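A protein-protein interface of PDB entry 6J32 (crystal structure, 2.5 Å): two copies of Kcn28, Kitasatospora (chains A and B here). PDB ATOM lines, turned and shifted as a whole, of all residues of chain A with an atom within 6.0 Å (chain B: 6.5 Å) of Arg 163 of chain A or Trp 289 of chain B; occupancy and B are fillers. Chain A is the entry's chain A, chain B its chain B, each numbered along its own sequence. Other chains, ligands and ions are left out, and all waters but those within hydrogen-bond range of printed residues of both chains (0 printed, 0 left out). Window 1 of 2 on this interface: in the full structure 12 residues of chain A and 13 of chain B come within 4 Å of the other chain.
OD1 of Asp 86 of chain A is in salt-bridge range of NH1 of Arg 163 of chain A (3.9 Å).
O of Ala 158 of chain A lies close to NE of Arg 162 of chain A (3.3 Å).
Among the printed residues, pairs that only touch across the chains: Arg 162 of chain A with Gly 222 of chain B (3.3 Å), Arg 163 of chain A with Gly 222 of chain B (3.5 Å), Arg 163 of chain A with Trp 289 of chain B (3.97 Å) and Ala 166 of chain A with Gly 222 of chain B (3.98 Å).
Printed residues of chain B within 4 Å of Arg 162 of chain A: Gly 222.
Printed residues of chain B within 4 Å of Ala 166 of chain A: Gly 222.
Of the printed residues of chain A, Gly 222 of chain B touches Arg 162 (3.3 Å), Arg 163 (3.5 Å) and Ala 166 (3.98 Å).
Gly 269 of chain B touches none of the printed residues of chain A.
Of chain A, only Arg 163 (3.97 Å) comes within 4 Å of Trp 289 of chain B.
The nearest residue of chain A that does not touch Trp 289 of chain B is Asp 82 of chain A (5.8 Å).
The nearest printed residue of chain B that does not touch Ala 166 of chain A is Gln 221 of chain B (5.2 Å).
Of the 15 printed residues of chain A, 3 touch a printed residue of chain B.
Printed residues of chain A that touch a printed residue of chain B: Arg 162, Arg 163 and Ala 166.
Hydrophobic or aromatic side chains of chain B that line the printed part of chain A: Trp 289.
No position is printed for both chains.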
ATOM      1  N   ASP A  82     -15.762  17.862  -5.229  1.00  0.00           N
ATOM      2  CA  ASP A  82     -16.906  18.558  -4.652  1.00  0.00           C
ATOM      3  C   ASP A  82     -16.522  19.283  -3.367  1.00  0.00           C
ATOM      4  O   ASP A  82     -16.948  20.422  -3.141  1.00  0.00           O
ATOM      5  CB  ASP A  82     -18.039  17.568  -4.381  1.00  0.00           C
ATOM      6  CG  ASP A  82     -18.794  17.184  -5.638  1.00  0.00           C
ATOM      7  OD1 ASP A  82     -18.873  18.016  -6.567  1.00  0.00           O
ATOM      8  OD2 ASP A  82     -19.314  16.048  -5.694  1.00  0.00           O
ATOM      9  N   LEU A  85     -14.511  22.429  -4.054  1.00  0.00           N
ATOM     10  CA  LEU A  85     -15.373  23.503  -4.532  1.00  0.00           C
ATOM     11  C   LEU A  85     -16.149  24.124  -3.379  1.00  0.00           C
ATOM     12  O   LEU A  85     -16.334  25.346  -3.335  1.00  0.00           O
ATOM     13  CB  LEU A  85     -16.323  22.980  -5.608  1.00  0.00           C
ATOM     14  CG  LEU A  85     -17.080  24.041  -6.409  1.00  0.00           C
ATOM     15  CD1 LEU A  85     -16.156  25.190  -6.797  1.00  0.00           C
ATOM     16  CD2 LEU A  85     -17.705  23.422  -7.649  1.00  0.00           C
ATOM     17  N   ASP A  86     -16.596  23.301  -2.428  1.00  0.00           N
ATOM     18  CA  ASP A  86     -17.303  23.829  -1.267  1.00  0.00           C
ATOM     19  C   ASP A  86     -16.420  24.794  -0.491  1.00  0.00           C
ATOM     20  O   ASP A  86     -16.885  25.843  -0.032  1.00  0.00           O
ATOM     21  CB  ASP A  86     -17.760  22.685  -0.362  1.00  0.00           C
ATOM     22  CG  ASP A  86     -18.733  21.746  -1.048  1.00  0.00           C
ATOM     23  OD1 ASP A  86     -19.451  22.195  -1.967  1.00  0.00           O
ATOM     24  OD2 ASP A  86     -18.777  20.555  -0.669  1.00  0.00           O
ATOM     25  N   VAL A  89     -16.225  28.048  -2.394  1.00  0.00           N
ATOM     26  CA  VAL A  89     -17.489  28.764  -2.261  1.00  0.00           C
ATOM     27  C   VAL A  89     -17.596  29.398  -0.883  1.00  0.00           C
ATOM     28  O   VAL A  89     -17.976  30.566  -0.748  1.00  0.00           O
ATOM     29  CB  VAL A  89     -18.668  27.810  -2.535  1.00  0.00           C
ATOM     30  CG1 VAL A  89     -19.993  28.466  -2.159  1.00  0.00           C
ATOM     31  CG2 VAL A  89     -18.677  27.378  -4.000  1.00  0.00           C
ATOM     32  N   ALA A 158     -20.071  16.863 -15.244  1.00  0.00           N
ATOM     33  CA  ALA A 158     -20.677  17.943 -16.013  1.00  0.00           C
ATOM     34  C   ALA A 158     -21.657  18.771 -15.200  1.00  0.00           C
ATOM     35  O   ALA A 158     -22.203  19.747 -15.719  1.00  0.00           O
ATOM     36  CB  ALA A 158     -21.379  17.382 -17.254  1.00  0.00           C
ATOM     37  N   ALA A 159     -21.873  18.415 -13.939  1.00  0.00           N
ATOM     38  CA  ALA A 159     -22.619  19.248 -13.008  1.00  0.00           C
ATOM     39  C   ALA A 159     -21.693  19.962 -12.042  1.00  0.00           C
ATOM     40  O   ALA A 159     -22.027  21.046 -11.556  1.00  0.00           O
ATOM     41  CB  ALA A 159     -23.633  18.407 -12.225  1.00  0.00           C
ATOM     42  N   HIS A 160     -20.537  19.356 -11.763  1.00  0.00           N
ATOM     43  CA  HIS A 160     -19.527  19.988 -10.924  1.00  0.00           C
ATOM     44  C   HIS A 160     -18.940  21.205 -11.632  1.00  0.00           C
ATOM     45  O   HIS A 160     -18.890  22.301 -11.064  1.00  0.00           O
ATOM     46  CB  HIS A 160     -18.449  18.964 -10.560  1.00  0.00           C
ATOM     47  CG  HIS A 160     -17.257  19.550  -9.873  1.00  0.00           C
ATOM     48  ND1 HIS A 160     -16.186  20.087 -10.555  1.00  0.00           N
ATOM     49  CD2 HIS A 160     -16.959  19.661  -8.557  1.00  0.00           C
ATOM     50  CE1 HIS A 160     -15.286  20.516  -9.688  1.00  0.00           C
ATOM     51  NE2 HIS A 160     -15.731  20.269  -8.468  1.00  0.00           N
ATOM     52  N   TYR A 161     -18.462  21.024 -12.872  1.00  0.00           N
ATOM     53  CA  TYR A 161     -17.954  22.156 -13.646  1.00  0.00           C
ATOM     54  C   TYR A 161     -19.026  23.217 -13.863  1.00  0.00           C
ATOM     55  O   TYR A 161     -18.740  24.417 -13.772  1.00  0.00           O
ATOM     56  CB  TYR A 161     -17.388  21.694 -14.991  1.00  0.00           C
ATOM     57  CG  TYR A 161     -15.983  21.130 -14.931  1.00  0.00           C
ATOM     58  CD1 TYR A 161     -14.886  21.949 -15.174  1.00  0.00           C
ATOM     59  CD2 TYR A 161     -15.748  19.793 -14.642  1.00  0.00           C
ATOM     60  CE1 TYR A 161     -13.597  21.458 -15.127  1.00  0.00           C
ATOM     61  CE2 TYR A 161     -14.456  19.289 -14.592  1.00  0.00           C
ATOM     62  CZ  TYR A 161     -13.386  20.128 -14.837  1.00  0.00           C
ATOM     63  OH  TYR A 161     -12.101  19.641 -14.790  1.00  0.00           O
ATOM     64  N   ARG A 162     -20.262  22.803 -14.163  1.00  0.00           N
ATOM     65  CA  ARG A 162     -21.342  23.777 -14.299  1.00  0.00           C
ATOM     66  C   ARG A 162     -21.506  24.575 -13.014  1.00  0.00           C
ATOM     67  O   ARG A 162     -21.723  25.792 -13.050  1.00  0.00           O
ATOM     68  CB  ARG A 162     -22.655  23.075 -14.650  1.00  0.00           C
ATOM     69  CG  ARG A 162     -22.852  22.754 -16.121  1.00  0.00           C
ATOM     70  CD  ARG A 162     -24.272  22.257 -16.365  1.00  0.00           C
ATOM     71  NE  ARG A 162     -24.374  21.394 -17.539  1.00  0.00           N
ATOM     72  CZ  ARG A 162     -24.443  21.830 -18.793  1.00  0.00           C
ATOM     73  NH1 ARG A 162     -24.423  23.131 -19.048  1.00  0.00           N
ATOM     74  NH2 ARG A 162     -24.533  20.962 -19.793  1.00  0.00           N
ATOM     75  N   ARG A 163     -21.393  23.900 -11.870  1.00  0.00           N
ATOM     76  CA  ARG A 163     -21.371  24.588 -10.584  1.00  0.00           C
ATOM     77  C   ARG A 163     -20.169  25.518 -10.480  1.00  0.00           C
ATOM     78  O   ARG A 163     -20.282  26.639  -9.969  1.00  0.00           O
ATOM     79  CB  ARG A 163     -21.367  23.548  -9.464  1.00  0.00           C
ATOM     80  CG  ARG A 163     -21.336  24.090  -8.059  1.00  0.00           C
ATOM     81  CD  ARG A 163     -21.766  22.997  -7.095  1.00  0.00           C
ATOM     82  NE  ARG A 163     -20.756  22.711  -6.084  1.00  0.00           N
ATOM     83  CZ  ARG A 163     -20.717  23.290  -4.890  1.00  0.00           C
ATOM     84  NH1 ARG A 163     -21.635  24.187  -4.556  1.00  0.00           N
ATOM     85  NH2 ARG A 163     -19.764  22.969  -4.030  1.00  0.00           N
ATOM     86  N   PHE A 164     -19.006  25.066 -10.956  1.00  0.00           N
ATOM     87  CA  PHE A 164     -17.813  25.906 -10.954  1.00  0.00           C
ATOM     88  C   PHE A 164     -18.007  27.117 -11.862  1.00  0.00           C
ATOM     89  O   PHE A 164     -17.728  28.256 -11.469  1.00  0.00           O
ATOM     90  CB  PHE A 164     -16.600  25.072 -11.384  1.00  0.00           C
ATOM     91  CG  PHE A 164     -15.274  25.587 -10.872  1.00  0.00           C
ATOM     92  CD1 PHE A 164     -15.048  26.942 -10.688  1.00  0.00           C
ATOM     93  CD2 PHE A 164     -14.251  24.700 -10.577  1.00  0.00           C
ATOM     94  CE1 PHE A 164     -13.828  27.403 -10.224  1.00  0.00           C
ATOM     95  CE2 PHE A 164     -13.029  25.155 -10.111  1.00  0.00           C
ATOM     96  CZ  PHE A 164     -12.818  26.507  -9.935  1.00  0.00           C
ATOM     97  N   ASP A 165     -18.494  26.886 -13.084  1.00  0.00           N
ATOM     98  CA  ASP A 165     -18.720  27.987 -14.017  1.00  0.00           C
ATOM     99  C   ASP A 165     -19.751  28.970 -13.478  1.00  0.00           C
ATOM    100  O   ASP A 165     -19.598  30.188 -13.630  1.00  0.00           O
ATOM    101  CB  ASP A 165     -19.175  27.444 -15.373  1.00  0.00           C
ATOM    102  CG  ASP A 165     -18.263  26.356 -15.907  1.00  0.00           C
ATOM    103  OD1 ASP A 165     -17.028  26.469 -15.749  1.00  0.00           O
ATOM    104  OD2 ASP A 165     -18.786  25.376 -16.478  1.00  0.00           O
ATOM    105  N   ALA A 166     -20.808  28.459 -12.839  1.00  0.00           N
ATOM    106  CA  ALA A 166     -21.827  29.337 -12.271  1.00  0.00           C
ATOM    107  C   ALA A 166     -21.255  30.203 -11.157  1.00  0.00           C
ATOM    108  O   ALA A 166     -21.606  31.382 -11.033  1.00  0.00           O
ATOM    109  CB  ALA A 166     -23.004  28.509 -11.754  1.00  0.00           C
ATOM    110  N   TRP A 167     -20.372  29.632 -10.335  1.00  0.00           N
ATOM    111  CA  TRP A 167     -19.763  30.398  -9.252  1.00  0.00           C
ATOM    112  C   TRP A 167     -18.907  31.540  -9.791  1.00  0.00           C
ATOM    113  O   TRP A 167     -18.890  32.634  -9.213  1.00  0.00           O
ATOM    114  CB  TRP A 167     -18.941  29.472  -8.356  1.00  0.00           C
ATOM    115  CG  TRP A 167     -18.199  30.185  -7.276  1.00  0.00           C
ATOM    116  CD1 TRP A 167     -18.738  30.906  -6.252  1.00  0.00           C
ATOM    117  CD2 TRP A 167     -16.780  30.230  -7.095  1.00  0.00           C
ATOM    118  NE1 TRP A 167     -17.742  31.408  -5.451  1.00  0.00           N
ATOM    119  CE2 TRP A 167     -16.530  31.005  -5.946  1.00  0.00           C
ATOM    120  CE3 TRP A 167     -15.697  29.689  -7.793  1.00  0.00           C
ATOM    121  CZ2 TRP A 167     -15.240  31.257  -5.482  1.00  0.00           C
ATOM    122  CZ3 TRP A 167     -14.417  29.942  -7.333  1.00  0.00           C
ATOM    123  CH2 TRP A 167     -14.200  30.718  -6.187  1.00  0.00           C
ATOM    124  N   LEU A 168     -18.182  31.307 -10.891  1.00  0.00           N
ATOM    125  CA  LEU A 168     -17.394  32.380 -11.492  1.00  0.00           C
ATOM    126  C   LEU A 168     -18.288  33.522 -11.958  1.00  0.00           C
ATOM    127  O   LEU A 168     -17.955  34.698 -11.771  1.00  0.00           O
ATOM    128  CB  LEU A 168     -16.564  31.848 -12.662  1.00  0.00           C
ATOM    129  CG  LEU A 168     -15.225  31.137 -12.432  1.00  0.00           C
ATOM    130  CD1 LEU A 168     -15.048  30.680 -10.996  1.00  0.00           C
ATOM    131  CD2 LEU A 168     -15.080  29.960 -13.387  1.00  0.00           C
ATOM    132  N   GLN B 221     -26.747  27.560  -8.346  1.00  0.00           N
ATOM    133  CA  GLN B 221     -26.360  26.288  -7.739  1.00  0.00           C
ATOM    134  C   GLN B 221     -25.762  25.338  -8.762  1.00  0.00           C
ATOM    135  O   GLN B 221     -25.607  24.142  -8.484  1.00  0.00           O
ATOM    136  CB  GLN B 221     -27.527  25.592  -7.025  1.00  0.00           C
ATOM    137  CG  GLN B 221     -27.526  25.694  -5.511  1.00  0.00           C
ATOM    138  CD  GLN B 221     -28.742  25.021  -4.901  1.00  0.00           C
ATOM    139  OE1 GLN B 221     -28.802  23.793  -4.802  1.00  0.00           O
ATOM    140  NE2 GLN B 221     -29.722  25.816  -4.507  1.00  0.00           N
ATOM    141  N   GLY B 222     -25.414  25.843  -9.946  1.00  0.00           N
ATOM    142  CA  GLY B 222     -24.823  25.053 -11.011  1.00  0.00           C
ATOM    143  C   GLY B 222     -25.684  24.975 -12.258  1.00  0.00           C
ATOM    144  O   GLY B 222     -25.159  24.745 -13.352  1.00  0.00           O
ATOM    145  N   ASP B 223     -26.997  25.155 -12.104  1.00  0.00           N
ATOM    146  CA  ASP B 223     -27.990  25.068 -13.174  1.00  0.00           C
ATOM    147  C   ASP B 223     -28.040  23.651 -13.741  1.00  0.00           C
ATOM    148  O   ASP B 223     -27.131  22.847 -13.516  1.00  0.00           O
ATOM    149  CB  ASP B 223     -27.714  26.102 -14.270  1.00  0.00           C
ATOM    150  CG  ASP B 223     -28.985  26.569 -14.960  1.00  0.00           C
ATOM    151  OD1 ASP B 223     -29.912  25.750 -15.122  1.00  0.00           O
ATOM    152  OD2 ASP B 223     -29.067  27.764 -15.318  1.00  0.00           O
ATOM    153  N   HIS B 241     -32.152  17.161   4.393  1.00  0.00           N
ATOM    154  CA  HIS B 241     -30.723  16.866   4.490  1.00  0.00           C
ATOM    155  C   HIS B 241     -30.351  15.390   4.637  1.00  0.00           C
ATOM    156  O   HIS B 241     -29.903  14.765   3.670  1.00  0.00           O
ATOM    157  CB  HIS B 241     -30.100  17.644   5.653  1.00  0.00           C
ATOM    158  CG  HIS B 241     -29.279  18.817   5.212  1.00  0.00           C
ATOM    159  ND1 HIS B 241     -28.881  18.990   3.904  1.00  0.00           N
ATOM    160  CD2 HIS B 241     -28.792  19.878   5.897  1.00  0.00           C
ATOM    161  CE1 HIS B 241     -28.179  20.104   3.803  1.00  0.00           C
ATOM    162  NE2 HIS B 241     -28.110  20.662   4.999  1.00  0.00           N
ATOM    163  N   LEU B 266     -31.438  11.150  -9.061  1.00  0.00           N
ATOM    164  CA  LEU B 266     -31.433  10.614  -7.705  1.00  0.00           C
ATOM    165  C   LEU B 266     -30.283  11.183  -6.883  1.00  0.00           C
ATOM    166  O   LEU B 266     -29.136  11.204  -7.342  1.00  0.00           O
ATOM    167  CB  LEU B 266     -31.343   9.087  -7.756  1.00  0.00           C
ATOM    168  CG  LEU B 266     -30.971   8.256  -6.525  1.00  0.00           C
ATOM    169  CD1 LEU B 266     -31.811   8.573  -5.305  1.00  0.00           C
ATOM    170  CD2 LEU B 266     -31.128   6.785  -6.892  1.00  0.00           C
ATOM    171  N   GLN B 267     -30.591  11.629  -5.662  1.00  0.00           N
ATOM    172  CA  GLN B 267     -29.597  12.111  -4.706  1.00  0.00           C
ATOM    173  C   GLN B 267     -29.490  11.088  -3.581  1.00  0.00           C
ATOM    174  O   GLN B 267     -30.426  10.924  -2.792  1.00  0.00           O
ATOM    175  CB  GLN B 267     -29.954  13.487  -4.149  1.00  0.00           C
ATOM    176  CG  GLN B 267     -29.077  13.893  -2.962  1.00  0.00           C
ATOM    177  CD  GLN B 267     -29.106  15.383  -2.668  1.00  0.00           C
ATOM    178  OE1 GLN B 267     -29.057  16.212  -3.578  1.00  0.00           O
ATOM    179  NE2 GLN B 267     -29.183  15.729  -1.389  1.00  0.00           N
ATOM    180  N   ILE B 268     -28.347  10.404  -3.510  1.00  0.00           N
ATOM    181  CA  ILE B 268     -28.163   9.361  -2.507  1.00  0.00           C
ATOM    182  C   ILE B 268     -27.663   9.884  -1.163  1.00  0.00           C
ATOM    183  O   ILE B 268     -27.931   9.254  -0.130  1.00  0.00           O
ATOM    184  CB  ILE B 268     -27.207   8.281  -3.045  1.00  0.00           C
ATOM    185  CG1 ILE B 268     -25.905   8.912  -3.536  1.00  0.00           C
ATOM    186  CG2 ILE B 268     -27.870   7.508  -4.176  1.00  0.00           C
ATOM    187  CD1 ILE B 268     -24.977   7.942  -4.236  1.00  0.00           C
ATOM    188  N   GLY B 269     -26.992  11.034  -1.132  1.00  0.00           N
ATOM    189  CA  GLY B 269     -26.573  11.623   0.129  1.00  0.00           C
ATOM    190  C   GLY B 269     -25.147  11.313   0.550  1.00  0.00           C
ATOM    191  O   GLY B 269     -24.633  10.219   0.292  1.00  0.00           O
ATOM    192  N   ARG B 270     -24.490  12.302   1.168  1.00  0.00           N
ATOM    193  CA  ARG B 270     -23.131  12.135   1.687  1.00  0.00           C
ATOM    194  C   ARG B 270     -22.964  10.871   2.531  1.00  0.00           C
ATOM    195  O   ARG B 270     -21.925  10.203   2.455  1.00  0.00           O
ATOM    196  CB  ARG B 270     -22.731  13.369   2.501  1.00  0.00           C
ATOM    197  CG  ARG B 270     -22.939  14.694   1.779  1.00  0.00           C
ATOM    198  CD  ARG B 270     -22.165  15.820   2.453  1.00  0.00           C
ATOM    199  NE  ARG B 270     -22.818  16.319   3.662  1.00  0.00           N
ATOM    200  CZ  ARG B 270     -23.459  17.480   3.738  1.00  0.00           C
ATOM    201  NH1 ARG B 270     -24.023  17.858   4.878  1.00  0.00           N
ATOM    202  NH2 ARG B 270     -23.529  18.270   2.674  1.00  0.00           N
ATOM    203  N   HIS B 287     -26.346  11.186  -7.867  1.00  0.00           N
ATOM    204  CA  HIS B 287     -25.398  12.041  -7.164  1.00  0.00           C
ATOM    205  C   HIS B 287     -25.560  11.862  -5.660  1.00  0.00           C
ATOM    206  O   HIS B 287     -26.601  11.412  -5.177  1.00  0.00           O
ATOM    207  CB  HIS B 287     -25.581  13.524  -7.512  1.00  0.00           C
ATOM    208  CG  HIS B 287     -25.145  13.882  -8.896  1.00  0.00           C
ATOM    209  ND1 HIS B 287     -25.901  13.600 -10.012  1.00  0.00           N
ATOM    210  CD2 HIS B 287     -24.031  14.509  -9.342  1.00  0.00           C
ATOM    211  CE1 HIS B 287     -25.269  14.033 -11.089  1.00  0.00           C
ATOM    212  NE2 HIS B 287     -24.132  14.589 -10.710  1.00  0.00           N
ATOM    213  N   ASN B 288     -24.510  12.228  -4.922  1.00  0.00           N
ATOM    214  CA  ASN B 288     -24.629  12.388  -3.478  1.00  0.00           C
ATOM    215  C   ASN B 288     -25.190  13.750  -3.108  1.00  0.00           C
ATOM    216  O   ASN B 288     -25.735  13.909  -2.009  1.00  0.00           O
ATOM    217  CB  ASN B 288     -23.273  12.196  -2.789  1.00  0.00           C
ATOM    218  CG  ASN B 288     -22.639  10.856  -3.098  1.00  0.00           C
ATOM    219  OD1 ASN B 288     -22.998   9.837  -2.505  1.00  0.00           O
ATOM    220  ND2 ASN B 288     -21.690  10.848  -4.027  1.00  0.00           N
ATOM    221  N   TRP B 289     -25.061  14.731  -3.998  1.00  0.00           N
ATOM    222  CA  TRP B 289     -25.649  16.047  -3.803  1.00  0.00           C
ATOM    223  C   TRP B 289     -25.939  16.620  -5.181  1.00  0.00           C
ATOM    224  O   TRP B 289     -25.063  16.615  -6.050  1.00  0.00           O
ATOM    225  CB  TRP B 289     -24.702  16.972  -3.031  1.00  0.00           C
ATOM    226  CG  TRP B 289     -25.242  18.355  -2.815  1.00  0.00           C
ATOM    227  CD1 TRP B 289     -25.907  18.810  -1.713  1.00  0.00           C
ATOM    228  CD2 TRP B 289     -25.187  19.456  -3.733  1.00  0.00           C
ATOM    229  NE1 TRP B 289     -26.252  20.128  -1.879  1.00  0.00           N
ATOM    230  CE2 TRP B 289     -25.827  20.547  -3.112  1.00  0.00           C
ATOM    231  CE3 TRP B 289     -24.654  19.626  -5.015  1.00  0.00           C
ATOM    232  CZ2 TRP B 289     -25.948  21.792  -3.730  1.00  0.00           C
ATOM    233  CZ3 TRP B 289     -24.778  20.862  -5.627  1.00  0.00           C
ATOM    234  CH2 TRP B 289     -25.418  21.928  -4.984  1.00  0.00           C
ATOM    235  N   VAL B 290     -27.160  17.111  -5.373  1.00  0.00           N
ATOM    236  CA  VAL B 290     -27.544  17.742  -6.633  1.00  0.00           C
ATOM    237  C   VAL B 290     -28.081  19.133  -6.317  1.00  0.00           C
ATOM    238  O   VAL B 290     -28.604  19.354  -5.215  1.00  0.00           O
ATOM    239  CB  VAL B 290     -28.570  16.891  -7.405  1.00  0.00           C
ATOM    240  CG1 VAL B 290     -28.698  15.508  -6.789  1.00  0.00           C
ATOM    241  CG2 VAL B 290     -29.925  17.579  -7.460  1.00  0.00           C
ATOM    242  N   PRO B 291     -27.960  20.096  -7.227  1.00  0.00           N
ATOM    243  CA  PRO B 291     -28.634  21.386  -7.025  1.00  0.00           C
ATOM    244  C   PRO B 291     -30.147  21.255  -7.084  1.00  0.00           C
ATOM    245  O   PRO B 291     -30.740  21.311  -8.168  1.00  0.00           O
ATOM    246  CB  PRO B 291     -28.099  22.254  -8.169  1.00  0.00           C
ATOM    247  CG  PRO B 291     -27.555  21.310  -9.177  1.00  0.00           C
ATOM    248  CD  PRO B 291     -27.167  20.052  -8.466  1.00  0.00           C
ATOM    249  N   GLN B 292     -30.774  21.072  -5.917  1.00  0.00           N
ATOM    250  CA  GLN B 292     -32.186  20.699  -5.869  1.00  0.00           C
ATOM    251  C   GLN B 292     -33.061  21.745  -6.544  1.00  0.00           C
ATOM    252  O   GLN B 292     -34.012  21.406  -7.259  1.00  0.00           O
ATOM    253  CB  GLN B 292     -32.617  20.503  -4.418  1.00  0.00           C
ATOM    254  CG  GLN B 292     -34.066  20.130  -4.246  1.00  0.00           C
ATOM    255  CD  GLN B 292     -34.409  19.848  -2.803  1.00  0.00           C
ATOM    256  OE1 GLN B 292     -34.476  18.693  -2.385  1.00  0.00           O
ATOM    257  NE2 GLN B 292     -34.633  20.903  -2.031  1.00  0.00           N
